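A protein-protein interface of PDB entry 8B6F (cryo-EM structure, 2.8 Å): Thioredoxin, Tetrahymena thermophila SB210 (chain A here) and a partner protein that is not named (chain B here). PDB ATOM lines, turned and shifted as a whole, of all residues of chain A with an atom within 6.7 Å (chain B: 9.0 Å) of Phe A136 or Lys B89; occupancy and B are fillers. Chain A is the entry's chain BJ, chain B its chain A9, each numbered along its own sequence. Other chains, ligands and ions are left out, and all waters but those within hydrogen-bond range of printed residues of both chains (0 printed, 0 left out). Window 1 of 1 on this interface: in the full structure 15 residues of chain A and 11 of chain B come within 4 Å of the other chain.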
ATOM      1  N   LYS A  44      -9.559   4.431  23.915  1.00  0.00           N
ATOM      2  CA  LYS A  44     -10.640   3.762  23.205  1.00  0.00           C
ATOM      3  C   LYS A  44     -11.822   3.501  24.129  1.00  0.00           C
ATOM      4  O   LYS A  44     -12.978   3.592  23.705  1.00  0.00           O
ATOM      5  CB  LYS A  44     -10.147   2.451  22.594  1.00  0.00           C
ATOM      6  CG  LYS A  44     -11.208   1.723  21.778  1.00  0.00           C
ATOM      7  CD  LYS A  44     -10.642   0.482  21.115  1.00  0.00           C
ATOM      8  CE  LYS A  44     -11.692  -0.221  20.272  1.00  0.00           C
ATOM      9  NZ  LYS A  44     -12.192   0.639  19.166  1.00  0.00           N
ATOM     10  N   CYS A 104     -16.685   5.461  24.451  1.00  0.00           N
ATOM     11  CA  CYS A 104     -16.042   4.646  23.426  1.00  0.00           C
ATOM     12  C   CYS A 104     -15.534   5.584  22.341  1.00  0.00           C
ATOM     13  O   CYS A 104     -16.328   6.205  21.629  1.00  0.00           O
ATOM     14  CB  CYS A 104     -17.011   3.622  22.842  1.00  0.00           C
ATOM     15  SG  CYS A 104     -16.342   2.717  21.432  1.00  0.00           S
ATOM     16  N   LEU A 105     -14.211   5.675  22.209  1.00  0.00           N
ATOM     17  CA  LEU A 105     -13.590   6.636  21.303  1.00  0.00           C
ATOM     18  C   LEU A 105     -14.062   8.051  21.623  1.00  0.00           C
ATOM     19  O   LEU A 105     -14.286   8.870  20.731  1.00  0.00           O
ATOM     20  CB  LEU A 105     -13.869   6.281  19.841  1.00  0.00           C
ATOM     21  CG  LEU A 105     -13.316   4.937  19.364  1.00  0.00           C
ATOM     22  CD1 LEU A 105     -13.802   4.629  17.959  1.00  0.00           C
ATOM     23  CD2 LEU A 105     -11.797   4.923  19.413  1.00  0.00           C
ATOM     24  N   GLY A 106     -14.218   8.339  22.913  1.00  0.00           N
ATOM     25  CA  GLY A 106     -14.642   9.656  23.336  1.00  0.00           C
ATOM     26  C   GLY A 106     -16.102   9.953  23.098  1.00  0.00           C
ATOM     27  O   GLY A 106     -16.498  11.120  23.124  1.00  0.00           O
ATOM     28  N   GLN A 107     -16.917   8.929  22.865  1.00  0.00           N
ATOM     29  CA  GLN A 107     -18.339   9.089  22.594  1.00  0.00           C
ATOM     30  C   GLN A 107     -19.129   8.367  23.674  1.00  0.00           C
ATOM     31  O   GLN A 107     -18.854   7.202  23.974  1.00  0.00           O
ATOM     32  CB  GLN A 107     -18.692   8.540  21.211  1.00  0.00           C
ATOM     33  CG  GLN A 107     -19.984   9.090  20.646  1.00  0.00           C
ATOM     34  CD  GLN A 107     -20.169   8.738  19.187  1.00  0.00           C
ATOM     35  OE1 GLN A 107     -19.573   7.789  18.685  1.00  0.00           O
ATOM     36  NE2 GLN A 107     -20.992   9.512  18.494  1.00  0.00           N
ATOM     37  N   VAL A 131     -18.219  -3.183  22.147  1.00  0.00           N
ATOM     38  CA  VAL A 131     -17.130  -2.572  21.391  1.00  0.00           C
ATOM     39  C   VAL A 131     -16.303  -3.644  20.698  1.00  0.00           C
ATOM     40  O   VAL A 131     -15.869  -3.473  19.553  1.00  0.00           O
ATOM     41  CB  VAL A 131     -16.275  -1.683  22.308  1.00  0.00           C
ATOM     42  CG1 VAL A 131     -14.974  -1.270  21.624  1.00  0.00           C
ATOM     43  CG2 VAL A 131     -17.078  -0.466  22.709  1.00  0.00           C
ATOM     44  N   LEU A 134     -18.129  -4.639  17.669  1.00  0.00           N
ATOM     45  CA  LEU A 134     -18.181  -3.614  16.636  1.00  0.00           C
ATOM     46  C   LEU A 134     -17.032  -3.773  15.648  1.00  0.00           C
ATOM     47  O   LEU A 134     -15.967  -4.301  15.973  1.00  0.00           O
ATOM     48  CB  LEU A 134     -18.123  -2.221  17.265  1.00  0.00           C
ATOM     49  CG  LEU A 134     -19.406  -1.686  17.904  1.00  0.00           C
ATOM     50  CD1 LEU A 134     -19.133  -0.367  18.600  1.00  0.00           C
ATOM     51  CD2 LEU A 134     -20.505  -1.519  16.868  1.00  0.00           C
ATOM     52  N   ASN A 135     -17.262  -3.301  14.421  1.00  0.00           N
ATOM     53  CA  ASN A 135     -16.249  -3.299  13.360  1.00  0.00           C
ATOM     54  C   ASN A 135     -16.308  -1.929  12.684  1.00  0.00           C
ATOM     55  O   ASN A 135     -17.084  -1.722  11.749  1.00  0.00           O
ATOM     56  CB  ASN A 135     -16.479  -4.429  12.364  1.00  0.00           C
ATOM     57  CG  ASN A 135     -16.388  -5.799  13.005  1.00  0.00           C
ATOM     58  OD1 ASN A 135     -17.354  -6.560  13.006  1.00  0.00           O
ATOM     59  ND2 ASN A 135     -15.220  -6.121  13.553  1.00  0.00           N
ATOM     60  N   PHE A 136     -15.485  -1.001  13.164  1.00  0.00           N
ATOM     61  CA  PHE A 136     -15.479   0.336  12.600  1.00  0.00           C
ATOM     62  C   PHE A 136     -14.782   0.340  11.241  1.00  0.00           C
ATOM     63  O   PHE A 136     -13.858  -0.443  11.007  1.00  0.00           O
ATOM     64  CB  PHE A 136     -14.770   1.313  13.532  1.00  0.00           C
ATOM     65  CG  PHE A 136     -15.511   1.586  14.807  1.00  0.00           C
ATOM     66  CD1 PHE A 136     -15.300   0.803  15.928  1.00  0.00           C
ATOM     67  CD2 PHE A 136     -16.405   2.640  14.888  1.00  0.00           C
ATOM     68  CE1 PHE A 136     -15.978   1.058  17.103  1.00  0.00           C
ATOM     69  CE2 PHE A 136     -17.085   2.901  16.059  1.00  0.00           C
ATOM     70  CZ  PHE A 136     -16.871   2.109  17.169  1.00  0.00           C
ATOM     71  N   PRO A 137     -15.202   1.212  10.325  1.00  0.00           N
ATOM     72  CA  PRO A 137     -14.458   1.365   9.071  1.00  0.00           C
ATOM     73  C   PRO A 137     -13.052   1.883   9.328  1.00  0.00           C
ATOM     74  O   PRO A 137     -12.803   2.630  10.275  1.00  0.00           O
ATOM     75  CB  PRO A 137     -15.292   2.379   8.277  1.00  0.00           C
ATOM     76  CG  PRO A 137     -16.649   2.312   8.872  1.00  0.00           C
ATOM     77  CD  PRO A 137     -16.445   2.005  10.323  1.00  0.00           C
ATOM     78  N   ALA A 138     -12.125   1.470   8.467  1.00  0.00           N
ATOM     79  CA  ALA A 138     -10.736   1.878   8.616  1.00  0.00           C
ATOM     80  C   ALA A 138     -10.593   3.374   8.370  1.00  0.00           C
ATOM     81  O   ALA A 138     -11.138   3.911   7.402  1.00  0.00           O
ATOM     82  CB  ALA A 138      -9.849   1.097   7.648  1.00  0.00           C
ATOM     83  N   GLY A 139      -9.855   4.046   9.250  1.00  0.00           N
ATOM     84  CA  GLY A 139      -9.606   5.465   9.116  1.00  0.00           C
ATOM     85  C   GLY A 139     -10.746   6.358   9.550  1.00  0.00           C
ATOM     86  O   GLY A 139     -10.640   7.582   9.402  1.00  0.00           O
ATOM     87  N   MET A 140     -11.830   5.793  10.081  1.00  0.00           N
ATOM     88  CA  MET A 140     -13.005   6.562  10.475  1.00  0.00           C
ATOM     89  C   MET A 140     -13.422   6.225  11.900  1.00  0.00           C
ATOM     90  O   MET A 140     -14.611   6.244  12.226  1.00  0.00           O
ATOM     91  CB  MET A 140     -14.159   6.310   9.506  1.00  0.00           C
ATOM     92  CG  MET A 140     -13.846   6.698   8.069  1.00  0.00           C
ATOM     93  SD  MET A 140     -14.938   5.915   6.870  1.00  0.00           S
ATOM     94  CE  MET A 140     -16.528   6.485   7.446  1.00  0.00           C
ATOM     95  N   ASP A 141     -12.454   5.910  12.760  1.00  0.00           N
ATOM     96  CA  ASP A 141     -12.716   5.552  14.149  1.00  0.00           C
ATOM     97  C   ASP A 141     -11.777   6.297  15.088  1.00  0.00           C
ATOM     98  O   ASP A 141     -11.381   5.766  16.128  1.00  0.00           O
ATOM     99  CB  ASP A 141     -12.593   4.044  14.355  1.00  0.00           C
ATOM    100  CG  ASP A 141     -11.253   3.502  13.904  1.00  0.00           C
ATOM    101  OD1 ASP A 141     -10.417   4.301  13.433  1.00  0.00           O
ATOM    102  OD2 ASP A 141     -11.036   2.278  14.020  1.00  0.00           O
ATOM    103  N   THR A 142     -11.408   7.521  14.731  1.00  0.00           N
ATOM    104  CA  THR A 142     -10.520   8.306  15.570  1.00  0.00           C
ATOM    105  C   THR A 142     -11.264   8.831  16.793  1.00  0.00           C
ATOM    106  O   THR A 142     -12.487   8.990  16.794  1.00  0.00           O
ATOM    107  CB  THR A 142      -9.928   9.474  14.782  1.00  0.00           C
ATOM    108  OG1 THR A 142     -10.983  10.318  14.304  1.00  0.00           O
ATOM    109  CG2 THR A 142      -9.115   8.964  13.601  1.00  0.00           C
ATOM    110  N   TYR A 143     -10.501   9.097  17.849  1.00  0.00           N
ATOM    111  CA  TYR A 143     -11.076   9.641  19.069  1.00  0.00           C
ATOM    112  C   TYR A 143     -11.680  11.016  18.809  1.00  0.00           C
ATOM    113  O   TYR A 143     -11.165  11.800  18.008  1.00  0.00           O
ATOM    114  CB  TYR A 143     -10.002   9.729  20.154  1.00  0.00           C
ATOM    115  CG  TYR A 143     -10.446  10.422  21.418  1.00  0.00           C
ATOM    116  CD1 TYR A 143     -10.283  11.790  21.574  1.00  0.00           C
ATOM    117  CD2 TYR A 143     -11.013   9.706  22.462  1.00  0.00           C
ATOM    118  CE1 TYR A 143     -10.681  12.428  22.728  1.00  0.00           C
ATOM    119  CE2 TYR A 143     -11.415  10.335  23.621  1.00  0.00           C
ATOM    120  CZ  TYR A 143     -11.247  11.696  23.746  1.00  0.00           C
ATOM    121  OH  TYR A 143     -11.644  12.331  24.898  1.00  0.00           O
ATOM    122  N   GLU A 144     -12.785  11.304  19.494  1.00  0.00           N
ATOM    123  CA  GLU A 144     -13.470  12.584  19.390  1.00  0.00           C
ATOM    124  C   GLU A 144     -13.740  13.124  20.786  1.00  0.00           C
ATOM    125  O   GLU A 144     -13.952  12.362  21.731  1.00  0.00           O
ATOM    126  CB  GLU A 144     -14.795  12.454  18.624  1.00  0.00           C
ATOM    127  CG  GLU A 144     -15.822  11.571  19.321  1.00  0.00           C
ATOM    128  CD  GLU A 144     -17.109  11.433  18.531  1.00  0.00           C
ATOM    129  OE1 GLU A 144     -17.189  11.992  17.419  1.00  0.00           O
ATOM    130  OE2 GLU A 144     -18.043  10.765  19.023  1.00  0.00           O
ATOM    131  N   GLN A 149     -20.277  15.276  19.295  1.00  0.00           N
ATOM    132  CA  GLN A 149     -21.559  14.742  18.845  1.00  0.00           C
ATOM    133  C   GLN A 149     -22.706  15.671  19.218  1.00  0.00           C
ATOM    134  O   GLN A 149     -23.611  15.903  18.409  1.00  0.00           O
ATOM    135  CB  GLN A 149     -21.787  13.349  19.429  1.00  0.00           C
ATOM    136  CG  GLN A 149     -23.041  12.664  18.907  1.00  0.00           C
ATOM    137  CD  GLN A 149     -23.011  12.460  17.406  1.00  0.00           C
ATOM    138  OE1 GLN A 149     -21.961  12.553  16.775  1.00  0.00           O
ATOM    139  NE2 GLN A 149     -24.173  12.187  16.824  1.00  0.00           N
ATOM    140  N   VAL B  82     -26.837  -0.491  10.081  1.00  0.00           N
ATOM    141  CA  VAL B  82     -25.499  -0.165  10.566  1.00  0.00           C
ATOM    142  C   VAL B  82     -25.608   0.275  12.021  1.00  0.00           C
ATOM    143  O   VAL B  82     -26.615   0.884  12.405  1.00  0.00           O
ATOM    144  CB  VAL B  82     -24.847   0.925   9.701  1.00  0.00           C
ATOM    145  CG1 VAL B  82     -23.400   1.138  10.104  1.00  0.00           C
ATOM    146  CG2 VAL B  82     -24.943   0.566   8.223  1.00  0.00           C
ATOM    147  N   PRO B  83     -24.616  -0.008  12.865  1.00  0.00           N
ATOM    148  CA  PRO B  83     -24.682   0.463  14.253  1.00  0.00           C
ATOM    149  C   PRO B  83     -24.733   1.980  14.324  1.00  0.00           C
ATOM    150  O   PRO B  83     -24.166   2.686  13.488  1.00  0.00           O
ATOM    151  CB  PRO B  83     -23.395  -0.086  14.878  1.00  0.00           C
ATOM    152  CG  PRO B  83     -23.051  -1.262  14.051  1.00  0.00           C
ATOM    153  CD  PRO B  83     -23.473  -0.915  12.655  1.00  0.00           C
ATOM    154  N   SER B  84     -25.431   2.481  15.345  1.00  0.00           N
ATOM    155  CA  SER B  84     -25.576   3.924  15.501  1.00  0.00           C
ATOM    156  C   SER B  84     -24.223   4.597  15.694  1.00  0.00           C
ATOM    157  O   SER B  84     -23.967   5.664  15.127  1.00  0.00           O
ATOM    158  CB  SER B  84     -26.493   4.234  16.683  1.00  0.00           C
ATOM    159  OG  SER B  84     -27.778   3.670  16.494  1.00  0.00           O
ATOM    160  N   ILE B  85     -23.341   3.983  16.483  1.00  0.00           N
ATOM    161  CA  ILE B  85     -22.027   4.574  16.724  1.00  0.00           C
ATOM    162  C   ILE B  85     -21.224   4.624  15.431  1.00  0.00           C
ATOM    163  O   ILE B  85     -20.532   5.610  15.153  1.00  0.00           O
ATOM    164  CB  ILE B  85     -21.287   3.801  17.832  1.00  0.00           C
ATOM    165  CG1 ILE B  85     -19.998   4.536  18.209  1.00  0.00           C
ATOM    166  CG2 ILE B  85     -20.981   2.377  17.391  1.00  0.00           C
ATOM    167  CD1 ILE B  85     -19.293   3.964  19.419  1.00  0.00           C
ATOM    168  N   VAL B  86     -21.295   3.565  14.626  1.00  0.00           N
ATOM    169  CA  VAL B  86     -20.587   3.561  13.349  1.00  0.00           C
ATOM    170  C   VAL B  86     -21.135   4.653  12.443  1.00  0.00           C
ATOM    171  O   VAL B  86     -20.376   5.359  11.769  1.00  0.00           O
ATOM    172  CB  VAL B  86     -20.685   2.172  12.691  1.00  0.00           C
ATOM    173  CG1 VAL B  86     -20.032   2.179  11.317  1.00  0.00           C
ATOM    174  CG2 VAL B  86     -20.041   1.122  13.581  1.00  0.00           C
ATOM    175  N   LEU B  87     -22.460   4.804  12.402  1.00  0.00           N
ATOM    176  CA  LEU B  87     -23.057   5.858  11.588  1.00  0.00           C
ATOM    177  C   LEU B  87     -22.600   7.235  12.050  1.00  0.00           C
ATOM    178  O   LEU B  87     -22.288   8.103  11.228  1.00  0.00           O
ATOM    179  CB  LEU B  87     -24.581   5.755  11.628  1.00  0.00           C
ATOM    180  CG  LEU B  87     -25.197   4.538  10.935  1.00  0.00           C
ATOM    181  CD1 LEU B  87     -26.691   4.484  11.188  1.00  0.00           C
ATOM    182  CD2 LEU B  87     -24.913   4.561   9.440  1.00  0.00           C
ATOM    183  N   LYS B  88     -22.568   7.461  13.363  1.00  0.00           N
ATOM    184  CA  LYS B  88     -22.117   8.750  13.875  1.00  0.00           C
ATOM    185  C   LYS B  88     -20.660   9.007  13.508  1.00  0.00           C
ATOM    186  O   LYS B  88     -20.298  10.123  13.118  1.00  0.00           O
ATOM    187  CB  LYS B  88     -22.304   8.806  15.389  1.00  0.00           C
ATOM    188  CG  LYS B  88     -23.756   8.795  15.833  1.00  0.00           C
ATOM    189  CD  LYS B  88     -23.864   8.816  17.346  1.00  0.00           C
ATOM    190  CE  LYS B  88     -25.310   8.847  17.805  1.00  0.00           C
ATOM    191  NZ  LYS B  88     -26.055   7.632  17.391  1.00  0.00           N
ATOM    192  N   LYS B  89     -19.808   7.989  13.636  1.00  0.00           N
ATOM    193  CA  LYS B  89     -18.398   8.164  13.306  1.00  0.00           C
ATOM    194  C   LYS B  89     -18.200   8.488  11.830  1.00  0.00           C
ATOM    195  O   LYS B  89     -17.400   9.363  11.483  1.00  0.00           O
ATOM    196  CB  LYS B  89     -17.613   6.907  13.681  1.00  0.00           C
ATOM    197  CG  LYS B  89     -17.422   6.711  15.175  1.00  0.00           C
ATOM    198  CD  LYS B  89     -16.483   7.754  15.758  1.00  0.00           C
ATOM    199  CE  LYS B  89     -16.222   7.491  17.229  1.00  0.00           C
ATOM    200  NZ  LYS B  89     -15.340   8.528  17.828  1.00  0.00           N
ATOM    201  N   MET B  90     -18.914   7.792  10.943  1.00  0.00           N
ATOM    202  CA  MET B  90     -18.744   8.055   9.518  1.00  0.00           C
ATOM    203  C   MET B  90     -19.323   9.408   9.127  1.00  0.00           C
ATOM    204  O   MET B  90     -18.775  10.078   8.247  1.00  0.00           O
ATOM    205  CB  MET B  90     -19.368   6.931   8.687  1.00  0.00           C
ATOM    206  CG  MET B  90     -20.833   6.679   8.938  1.00  0.00           C
ATOM    207  SD  MET B  90     -21.337   5.032   8.394  1.00  0.00           S
ATOM    208  CE  MET B  90     -20.917   5.094   6.658  1.00  0.00           C
ATOM    209  N   PHE B  91     -20.415   9.834   9.765  1.00  0.00           N
ATOM    210  CA  PHE B  91     -20.924  11.182   9.524  1.00  0.00           C
ATOM    211  C   PHE B  91     -19.928  12.230   9.999  1.00  0.00           C
ATOM    212  O   PHE B  91     -19.738  13.259   9.342  1.00  0.00           O
ATOM    213  CB  PHE B  91     -22.278  11.380  10.207  1.00  0.00           C
ATOM    214  CG  PHE B  91     -23.346  10.433   9.731  1.00  0.00           C
ATOM    215  CD1 PHE B  91     -23.223   9.764   8.521  1.00  0.00           C
ATOM    216  CD2 PHE B  91     -24.480  10.218  10.494  1.00  0.00           C
ATOM    217  CE1 PHE B  91     -24.206   8.899   8.089  1.00  0.00           C
ATOM    218  CE2 PHE B  91     -25.465   9.353  10.067  1.00  0.00           C
ATOM    219  CZ  PHE B  91     -25.329   8.693   8.862  1.00  0.00           C
ATOM    220  N   ARG B  92     -19.279  11.983  11.137  1.00  0.00           N
ATOM    221  CA  ARG B  92     -18.229  12.884  11.599  1.00  0.00           C
ATOM    222  C   ARG B  92     -17.086  12.942  10.597  1.00  0.00           C
ATOM    223  O   ARG B  92     -16.511  14.009  10.362  1.00  0.00           O
ATOM    224  CB  ARG B  92     -17.718  12.444  12.970  1.00  0.00           C
ATOM    225  CG  ARG B  92     -16.465  13.180  13.413  1.00  0.00           C
ATOM    226  CD  ARG B  92     -16.161  12.921  14.877  1.00  0.00           C
ATOM    227  NE  ARG B  92     -14.922  13.561  15.301  1.00  0.00           N
ATOM    228  CZ  ARG B  92     -13.720  13.006  15.217  1.00  0.00           C
ATOM    229  NH1 ARG B  92     -13.550  11.791  14.723  1.00  0.00           N
ATOM    230  NH2 ARG B  92     -12.661  13.689  15.642  1.00  0.00           N
ATOM    231  N   PHE B  93     -16.736  11.801  10.004  1.00  0.00           N
ATOM    232  CA  PHE B  93     -15.717  11.800   8.961  1.00  0.00           C
ATOM    233  C   PHE B  93     -16.139  12.668   7.783  1.00  0.00           C
ATOM    234  O   PHE B  93     -15.328  13.428   7.243  1.00  0.00           O
ATOM    235  CB  PHE B  93     -15.443  10.368   8.498  1.00  0.00           C
ATOM    236  CG  PHE B  93     -14.573  10.288   7.280  1.00  0.00           C
ATOM    237  CD1 PHE B  93     -13.194  10.282   7.399  1.00  0.00           C
ATOM    238  CD2 PHE B  93     -15.132  10.226   6.016  1.00  0.00           C
ATOM    239  CE1 PHE B  93     -12.389  10.212   6.282  1.00  0.00           C
ATOM    240  CE2 PHE B  93     -14.332  10.157   4.894  1.00  0.00           C
ATOM    241  CZ  PHE B  93     -12.959  10.151   5.028  1.00  0.00           C
ATOM    242  N   VAL B  94     -17.404  12.572   7.369  1.00  0.00           N
ATOM    243  CA  VAL B  94     -17.894  13.418   6.283  1.00  0.00           C
ATOM    244  C   VAL B  94     -17.736  14.886   6.649  1.00  0.00           C
ATOM    245  O   VAL B  94     -17.292  15.700   5.831  1.00  0.00           O
ATOM    246  CB  VAL B  94     -19.359  13.077   5.952  1.00  0.00           C
ATOM    247  CG1 VAL B  94     -19.907  14.021   4.890  1.00  0.00           C
ATOM    248  CG2 VAL B  94     -19.479  11.648   5.486  1.00  0.00           C
ATOM    249  N   ARG B  95     -18.104  15.251   7.877  1.00  0.00           N
ATOM    250  CA  ARG B  95     -17.994  16.646   8.288  1.00  0.00           C
ATOM    251  C   ARG B  95     -16.545  17.113   8.265  1.00  0.00           C
ATOM    252  O   ARG B  95     -16.255  18.239   7.848  1.00  0.00           O
ATOM    253  CB  ARG B  95     -18.587  16.832   9.686  1.00  0.00           C
ATOM    254  CG  ARG B  95     -20.071  16.519   9.785  1.00  0.00           C
ATOM    255  CD  ARG B  95     -20.670  17.112  11.045  1.00  0.00           C
ATOM    256  NE  ARG B  95     -19.842  16.861  12.219  1.00  0.00           N
ATOM    257  CZ  ARG B  95     -19.935  15.789  12.996  1.00  0.00           C
ATOM    258  NH1 ARG B  95     -20.808  14.827  12.749  1.00  0.00           N
ATOM    259  NH2 ARG B  95     -19.130  15.681  14.049  1.00  0.00           N
ATOM    260  N   ASN B  96     -15.620  16.264   8.713  1.00  0.00           N
ATOM    261  CA  ASN B  96     -14.227  16.654   8.872  1.00  0.00           C
ATOM    262  C   ASN B  96     -13.390  16.477   7.611  1.00  0.00           C
ATOM    263  O   ASN B  96     -12.228  16.895   7.603  1.00  0.00           O
ATOM    264  CB  ASN B  96     -13.586  15.848  10.005  1.00  0.00           C
ATOM    265  CG  ASN B  96     -14.257  16.083  11.340  1.00  0.00           C
ATOM    266  OD1 ASN B  96     -15.363  16.616  11.406  1.00  0.00           O
ATOM    267  ND2 ASN B  96     -13.591  15.682  12.415  1.00  0.00           N
ATOM    268  N   ASN B  97     -13.933  15.871   6.558  1.00  0.00           N
ATOM    269  CA  ASN B  97     -13.179  15.615   5.338  1.00  0.00           C
ATOM    270  C   ASN B  97     -14.000  16.002   4.119  1.00  0.00           C
ATOM    271  O   ASN B  97     -15.194  15.702   4.042  1.00  0.00           O
ATOM    272  CB  ASN B  97     -12.774  14.140   5.234  1.00  0.00           C
ATOM    273  CG  ASN B  97     -11.958  13.677   6.422  1.00  0.00           C
ATOM    274  OD1 ASN B  97     -12.505  13.224   7.426  1.00  0.00           O
ATOM    275  ND2 ASN B  97     -10.640  13.790   6.314  1.00  0.00           N
ATOM    276  N   ILE B 104     -16.990   7.006   1.921  1.00  0.00           N
ATOM    277  CA  ILE B 104     -18.000   6.165   2.559  1.00  0.00           C
ATOM    278  C   ILE B 104     -18.616   5.220   1.538  1.00  0.00           C
ATOM    279  O   ILE B 104     -18.832   4.035   1.817  1.00  0.00           O
ATOM    280  CB  ILE B 104     -19.068   7.028   3.255  1.00  0.00           C
ATOM    281  CG1 ILE B 104     -18.462   7.696   4.489  1.00  0.00           C
ATOM    282  CG2 ILE B 104     -20.284   6.176   3.626  1.00  0.00           C
ATOM    283  CD1 ILE B 104     -19.439   8.490   5.320  1.00  0.00           C
ATOM    284  N   ASP B 107     -16.158   2.441   0.870  1.00  0.00           N
ATOM    285  CA  ASP B 107     -16.131   1.461   1.952  1.00  0.00           C
ATOM    286  C   ASP B 107     -17.364   0.567   1.929  1.00  0.00           C
ATOM    287  O   ASP B 107     -17.264  -0.645   2.151  1.00  0.00           O
ATOM    288  CB  ASP B 107     -16.026   2.176   3.298  1.00  0.00           C
ATOM    289  CG  ASP B 107     -14.771   3.015   3.415  1.00  0.00           C
ATOM    290  OD1 ASP B 107     -13.714   2.580   2.913  1.00  0.00           O
ATOM    291  OD2 ASP B 107     -14.842   4.111   4.008  1.00  0.00           O
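Printed residues of chain A that touch a printed residue of chain B: Cys A104, Leu A105, Gln A107, Leu A134, Phe A136, Pro A137, Met A140, Thr A142, Tyr A143, Glu A144 and Gln A149. Along chain B the printed residues that touch a printed residue of chain A span positions 83 to 107. Among the printed residues, Asp or Glu carboxylates within 4 Å of a Lys or Arg side-chain nitrogen of the other chain: Glu A144 with Lys B89 and Glu A144 with Arg B92.
Of chain B, only Ile B85 and Lys B89 come within 4 Å of Phe A136. Lys B89 touches just these residues of chain A: Leu A105 (3.1 Å), Gln A107 (3.7 Å), Phe A136 (3.9 Å), Met A140 (3.4 Å), Thr A142 (3.1 Å) and Glu A144 (3.4 Å). Pro A137 touches one residue of chain B. Of the printed residues of chain B, Gln A149 touches Lys B88. Of the printed residues of chain A, Met B90 touches Met A140 (3.1 Å). Printed residues of chain A within 4 Å of Ile B85: Cys A104 (3.8 Å), Gln A107 (3.3 Å), Leu A134 (3.5 Å) and Phe A136 (3.8 Å). Of the printed residues of chain B, Leu A105 touches Lys B89. Of the printed residues of chain B, Met A140 touches Lys B89 (3.4 Å), Met B90 (3.1 Å), Phe B93 (3.7 Å), Ile B104 (3.7 Å) and Asp B107 (3.4 Å). Asn A135 touches none of the printed residues of chain B. Lys A44 touches none of the printed residues of chain B. The nearest residue of chain B that does not touch Phe A136 is Val B86 (4.2 Å). The nearest printed residue of chain A that does not touch Lys B89 is Tyr A143 (4.5 Å).
Cys A104 touches Ile B85. OE1 of Gln A107 touches CG1 of Ile B85, at 3.3 Å. Gln A107 touches Lys B88 (NE2 to CD, 3.2 Å). Gln A107 touches Lys B89 (OE1 to CE, 3.7 Å). Leu A134 touches Pro B83 (CD2 to CB, 3.8 Å). CD1 of Ile B85 touches CZ of Phe A136, at 3.8 Å. Pro A137 touches Val B86. CB of Lys B89 touches O of Met A140 (3.4 Å). CG of Met A140 touches CD1 of Phe B93 (3.7 Å). Ile B104 touches Met A140 (CG1 to CE, 3.7 Å).
The backbone carbonyl oxygen of Arg B92 sits close to the side-chain amide oxygen of Asn B96. The backbone NH of Glu A144 sits at hydrogen-bond distance from the backbone carbonyl oxygen of Leu A105, 3.1 Å away. The backbone NH (N) of Leu A105 lies within hydrogen-bond range of the backbone carbonyl oxygen (O) of Lys A44 (2.8 Å). O of Phe B93 sits close to OD1 of Asn B97, 2.8 Å away. OE2 of Glu A144 lies close to NE2 of Gln A107 (3.2 Å).
O of Thr A142 is in hydrogen-bond range of NZ of Lys B89, 3.1 Å away. NH2 of Arg B92 is in hydrogen-bond range of O of Tyr A143, 3.4 Å away. OD2 of Asp B107 sits close to SD of Met A140 (3.4 Å). NZ of Lys B89 is in hydrogen-bond range of O of Leu A105. The guanidinium group (NE) of Arg B92 lies within salt-bridge range of the side-chain carboxylate (OE1) of Glu A144, at 3.5 Å. OE2 of Glu A144 is in salt-bridge range of NZ of Lys B89, at 3.7 Å. The guanidinium group of Arg B92 is in hydrogen-bond range of the side-chain hydroxyl of Thr A142 (3.0 Å).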
